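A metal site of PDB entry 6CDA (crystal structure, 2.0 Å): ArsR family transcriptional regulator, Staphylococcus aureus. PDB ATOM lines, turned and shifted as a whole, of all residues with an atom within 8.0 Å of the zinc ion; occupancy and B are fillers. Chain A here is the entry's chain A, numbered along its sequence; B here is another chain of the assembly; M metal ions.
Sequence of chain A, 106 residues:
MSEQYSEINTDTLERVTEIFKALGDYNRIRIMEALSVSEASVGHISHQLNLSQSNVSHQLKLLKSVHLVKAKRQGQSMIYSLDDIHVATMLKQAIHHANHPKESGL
The zinc ion is bound by a ring nitrogen (NE2) of His 100 of chain B (1.9 Å), the side-chain carboxylate (OD1) of Asp 84 (2.0 Å), a ring nitrogen (ND1) of His 86 (2.1 Å) and a ring nitrogen (ND1) of His 97 of chain B (2.2 Å).
Slightly farther from the zinc ion lies the side-chain carboxylate (OD2) of Asp 84 (2.8 Å).
Within 4 Å of the zinc ion: Asp 84, His 86, His 97 of chain B and His 100 of chain B.
The nearest printed residue that does not touch the zinc ion is Asp 83 (4.8 Å).
OD2 of Asp 84 is in hydrogen-bond range of N of Val 87, 3.4 Å away.
A ring nitrogen (NE2) of His 97 of chain B is in hydrogen-bond range of the backbone carbonyl oxygen (O) of His 67 (2.7 Å).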
ATOM      1  N   HIS A  67      14.492   4.757 -18.415  1.00  0.00           N
ATOM      2  CA  HIS A  67      13.903   3.472 -18.727  1.00  0.00           C
ATOM      3  C   HIS A  67      12.392   3.475 -18.567  1.00  0.00           C
ATOM      4  O   HIS A  67      11.789   2.469 -18.227  1.00  0.00           O
ATOM      5  CB  HIS A  67      14.577   2.386 -17.895  1.00  0.00           C
ATOM      6  CG  HIS A  67      16.013   2.178 -18.297  1.00  0.00           C
ATOM      7  ND1 HIS A  67      17.076   2.436 -17.457  1.00  0.00           N
ATOM      8  CD2 HIS A  67      16.549   1.857 -19.499  1.00  0.00           C
ATOM      9  CE1 HIS A  67      18.196   2.204 -18.111  1.00  0.00           C
ATOM     10  NE2 HIS A  67      17.905   1.861 -19.354  1.00  0.00           N
ATOM     11  N   ASP A  83       8.139   1.253 -21.513  1.00  0.00           N
ATOM     12  CA  ASP A  83       9.205   0.272 -21.430  1.00  0.00           C
ATOM     13  C   ASP A  83       8.677  -1.113 -21.159  1.00  0.00           C
ATOM     14  O   ASP A  83       8.986  -2.043 -21.908  1.00  0.00           O
ATOM     15  CB  ASP A  83      10.197   0.661 -20.350  1.00  0.00           C
ATOM     16  CG  ASP A  83      11.351  -0.336 -20.268  1.00  0.00           C
ATOM     17  OD1 ASP A  83      12.298  -0.244 -21.102  1.00  0.00           O
ATOM     18  OD2 ASP A  83      11.284  -1.226 -19.396  1.00  0.00           O
ATOM     19  N   ASP A  84       7.913  -1.293 -20.083  1.00  0.00           N
ATOM     20  CA  ASP A  84       7.390  -2.609 -19.734  1.00  0.00           C
ATOM     21  C   ASP A  84       6.117  -2.450 -18.891  1.00  0.00           C
ATOM     22  O   ASP A  84       5.596  -1.337 -18.703  1.00  0.00           O
ATOM     23  CB  ASP A  84       8.472  -3.472 -19.050  1.00  0.00           C
ATOM     24  CG  ASP A  84       8.754  -3.088 -17.618  1.00  0.00           C
ATOM     25  OD1 ASP A  84       9.749  -3.642 -17.086  1.00  0.00           O
ATOM     26  OD2 ASP A  84       8.008  -2.261 -17.010  1.00  0.00           O
ATOM     27  N   ILE A  85       5.608  -3.575 -18.387  1.00  0.00           N
ATOM     28  CA  ILE A  85       4.307  -3.583 -17.732  1.00  0.00           C
ATOM     29  C   ILE A  85       4.337  -2.790 -16.441  1.00  0.00           C
ATOM     30  O   ILE A  85       3.309  -2.275 -16.000  1.00  0.00           O
ATOM     31  CB  ILE A  85       3.846  -5.020 -17.443  1.00  0.00           C
ATOM     32  CG1 ILE A  85       2.415  -5.034 -16.941  1.00  0.00           C
ATOM     33  CG2 ILE A  85       4.707  -5.649 -16.338  1.00  0.00           C
ATOM     34  CD1 ILE A  85       1.417  -4.534 -17.965  1.00  0.00           C
ATOM     35  N   HIS A  86       5.503  -2.715 -15.805  1.00  0.00           N
ATOM     36  CA  HIS A  86       5.625  -1.932 -14.585  1.00  0.00           C
ATOM     37  C   HIS A  86       5.303  -0.477 -14.832  1.00  0.00           C
ATOM     38  O   HIS A  86       4.656   0.194 -14.007  1.00  0.00           O
ATOM     39  CB  HIS A  86       7.032  -2.052 -14.018  1.00  0.00           C
ATOM     40  CG  HIS A  86       7.408  -3.451 -13.626  1.00  0.00           C
ATOM     41  ND1 HIS A  86       8.615  -4.002 -13.968  1.00  0.00           N
ATOM     42  CD2 HIS A  86       6.753  -4.395 -12.902  1.00  0.00           C
ATOM     43  CE1 HIS A  86       8.692  -5.230 -13.482  1.00  0.00           C
ATOM     44  NE2 HIS A  86       7.571  -5.490 -12.840  1.00  0.00           N
ATOM     45  N   VAL A  87       5.779   0.056 -15.951  1.00  0.00           N
ATOM     46  CA  VAL A  87       5.566   1.453 -16.286  1.00  0.00           C
ATOM     47  C   VAL A  87       4.103   1.688 -16.612  1.00  0.00           C
ATOM     48  O   VAL A  87       3.474   2.654 -16.138  1.00  0.00           O
ATOM     49  CB  VAL A  87       6.487   1.839 -17.446  1.00  0.00           C
ATOM     50  CG1 VAL A  87       6.322   3.291 -17.798  1.00  0.00           C
ATOM     51  CG2 VAL A  87       7.932   1.540 -17.069  1.00  0.00           C
ATOM     52  N   ALA A  88       3.512   0.759 -17.360  1.00  0.00           N
ATOM     53  CA  ALA A  88       2.106   0.874 -17.696  1.00  0.00           C
ATOM     54  C   ALA A  88       1.251   0.878 -16.444  1.00  0.00           C
ATOM     55  O   ALA A  88       0.351   1.724 -16.294  1.00  0.00           O
ATOM     56  CB  ALA A  88       1.704  -0.293 -18.618  1.00  0.00           C
ATOM     57  N   GLN B  93       5.354  -0.833  -7.986  1.00  0.00           N
ATOM     58  CA  GLN B  93       5.753  -1.101  -9.364  1.00  0.00           C
ATOM     59  C   GLN B  93       6.998  -0.309  -9.742  1.00  0.00           C
ATOM     60  O   GLN B  93       7.900  -0.833 -10.396  1.00  0.00           O
ATOM     61  CB  GLN B  93       4.576  -0.802 -10.287  1.00  0.00           C
ATOM     62  CG  GLN B  93       3.409  -1.812 -10.064  1.00  0.00           C
ATOM     63  CD  GLN B  93       3.676  -3.165 -10.711  1.00  0.00           C
ATOM     64  OE1 GLN B  93       3.616  -4.224 -10.074  1.00  0.00           O
ATOM     65  NE2 GLN B  93       3.958  -3.136 -11.981  1.00  0.00           N
ATOM     66  N   ALA B  94       7.064   0.938  -9.309  1.00  0.00           N
ATOM     67  CA  ALA B  94       8.253   1.765  -9.533  1.00  0.00           C
ATOM     68  C   ALA B  94       9.504   1.110  -8.971  1.00  0.00           C
ATOM     69  O   ALA B  94      10.553   1.054  -9.639  1.00  0.00           O
ATOM     70  CB  ALA B  94       8.006   3.132  -8.915  1.00  0.00           C
ATOM     71  N   ILE B  95       9.421   0.593  -7.743  1.00  0.00           N
ATOM     72  CA  ILE B  95      10.579  -0.044  -7.131  1.00  0.00           C
ATOM     73  C   ILE B  95      10.940  -1.343  -7.841  1.00  0.00           C
ATOM     74  O   ILE B  95      12.113  -1.618  -8.126  1.00  0.00           O
ATOM     75  CB  ILE B  95      10.324  -0.237  -5.621  1.00  0.00           C
ATOM     76  CG1 ILE B  95      10.179   1.130  -4.973  1.00  0.00           C
ATOM     77  CG2 ILE B  95      11.488  -0.943  -4.965  1.00  0.00           C
ATOM     78  CD1 ILE B  95       9.681   1.063  -3.511  1.00  0.00           C
ATOM     79  N   HIS B  96       9.936  -2.174  -8.152  1.00  0.00           N
ATOM     80  CA  HIS B  96      10.176  -3.331  -9.030  1.00  0.00           C
ATOM     81  C   HIS B  96      10.964  -2.935 -10.263  1.00  0.00           C
ATOM     82  O   HIS B  96      11.905  -3.629 -10.666  1.00  0.00           O
ATOM     83  CB  HIS B  96       8.839  -3.945  -9.502  1.00  0.00           C
ATOM     84  CG  HIS B  96       8.265  -4.977  -8.576  1.00  0.00           C
ATOM     85  ND1 HIS B  96       6.912  -5.046  -8.306  1.00  0.00           N
ATOM     86  CD2 HIS B  96       8.834  -6.010  -7.917  1.00  0.00           C
ATOM     87  CE1 HIS B  96       6.678  -6.061  -7.497  1.00  0.00           C
ATOM     88  NE2 HIS B  96       7.826  -6.663  -7.249  1.00  0.00           N
ATOM     89  N   HIS B  97      10.537  -1.851 -10.930  1.00  0.00           N
ATOM     90  CA  HIS B  97      11.109  -1.512 -12.243  1.00  0.00           C
ATOM     91  C   HIS B  97      12.551  -1.056 -12.086  1.00  0.00           C
ATOM     92  O   HIS B  97      13.404  -1.356 -12.925  1.00  0.00           O
ATOM     93  CB  HIS B  97      10.276  -0.431 -12.920  1.00  0.00           C
ATOM     94  CG  HIS B  97      10.719  -0.093 -14.306  1.00  0.00           C
ATOM     95  ND1 HIS B  97      10.636  -0.989 -15.357  1.00  0.00           N
ATOM     96  CD2 HIS B  97      11.190   1.061 -14.835  1.00  0.00           C
ATOM     97  CE1 HIS B  97      11.065  -0.407 -16.462  1.00  0.00           C
ATOM     98  NE2 HIS B  97      11.406   0.837 -16.173  1.00  0.00           N
ATOM     99  N   ALA B  98      12.819  -0.294 -11.032  1.00  0.00           N
ATOM    100  CA  ALA B  98      14.149   0.156 -10.654  1.00  0.00           C
ATOM    101  C   ALA B  98      15.086  -0.969 -10.297  1.00  0.00           C
ATOM    102  O   ALA B  98      16.284  -0.724 -10.227  1.00  0.00           O
ATOM    103  CB  ALA B  98      14.072   1.089  -9.450  1.00  0.00           C
ATOM    104  N   ASN B  99      14.596  -2.180 -10.080  1.00  0.00           N
ATOM    105  CA  ASN B  99      15.450  -3.246  -9.572  1.00  0.00           C
ATOM    106  C   ASN B  99      15.672  -4.383 -10.554  1.00  0.00           C
ATOM    107  O   ASN B  99      16.235  -5.416 -10.177  1.00  0.00           O
ATOM    108  CB  ASN B  99      14.886  -3.790  -8.251  1.00  0.00           C
ATOM    109  CG  ASN B  99      15.593  -3.215  -7.045  1.00  0.00           C
ATOM    110  OD1 ASN B  99      16.727  -2.738  -7.141  1.00  0.00           O
ATOM    111  ND2 ASN B  99      14.927  -3.257  -5.893  1.00  0.00           N
ATOM    112  N   HIS B 100      15.240  -4.246 -11.799  1.00  0.00           N
ATOM    113  CA  HIS B 100      15.562  -5.301 -12.753  1.00  0.00           C
ATOM    114  C   HIS B 100      16.412  -4.723 -13.866  1.00  0.00           C
ATOM    115  O   HIS B 100      16.634  -3.514 -13.889  1.00  0.00           O
ATOM    116  CB  HIS B 100      14.292  -5.982 -13.276  1.00  0.00           C
ATOM    117  CG  HIS B 100      13.364  -5.113 -14.065  1.00  0.00           C
ATOM    118  ND1 HIS B 100      13.558  -4.833 -15.404  1.00  0.00           N
ATOM    119  CD2 HIS B 100      12.177  -4.557 -13.732  1.00  0.00           C
ATOM    120  CE1 HIS B 100      12.554  -4.098 -15.844  1.00  0.00           C
ATOM    121  NE2 HIS B 100      11.700  -3.913 -14.850  1.00  0.00           N
ATOM    122  N   PRO B 101      16.936  -5.560 -14.768  1.00  0.00           N
ATOM    123  CA  PRO B 101      17.739  -5.069 -15.893  1.00  0.00           C
ATOM    124  C   PRO B 101      16.917  -4.613 -17.088  1.00  0.00           C
ATOM    125  O   PRO B 101      15.794  -5.066 -17.314  1.00  0.00           O
ATOM    126  CB  PRO B 101      18.586  -6.301 -16.285  1.00  0.00           C
ATOM    127  CG  PRO B 101      18.399  -7.315 -15.190  1.00  0.00           C
ATOM    128  CD  PRO B 101      17.077  -7.019 -14.589  1.00  0.00           C
ATOM    129  N   LYS B 102      17.533  -3.728 -17.885  1.00  0.00           N
ATOM    130  CA  LYS B 102      17.000  -3.300 -19.191  1.00  0.00           C
ATOM    131  C   LYS B 102      15.780  -2.391 -19.055  1.00  0.00           C
ATOM    132  O   LYS B 102      15.204  -1.977 -20.063  1.00  0.00           O
ATOM    133  CB  LYS B 102      16.629  -4.508 -20.078  1.00  0.00           C
ATOM    134  CG  LYS B 102      17.805  -5.249 -20.626  1.00  0.00           C
ATOM    135  CD  LYS B 102      17.331  -6.263 -21.601  1.00  0.00           C
ATOM    136  CE  LYS B 102      18.318  -6.462 -22.752  1.00  0.00           C
ATOM    137  NZ  LYS B 102      18.005  -5.687 -24.019  1.00  0.00           N
HETATM  138 ZN    ZN M   1       9.995  -3.060 -15.192  1.00  0.00          ZN
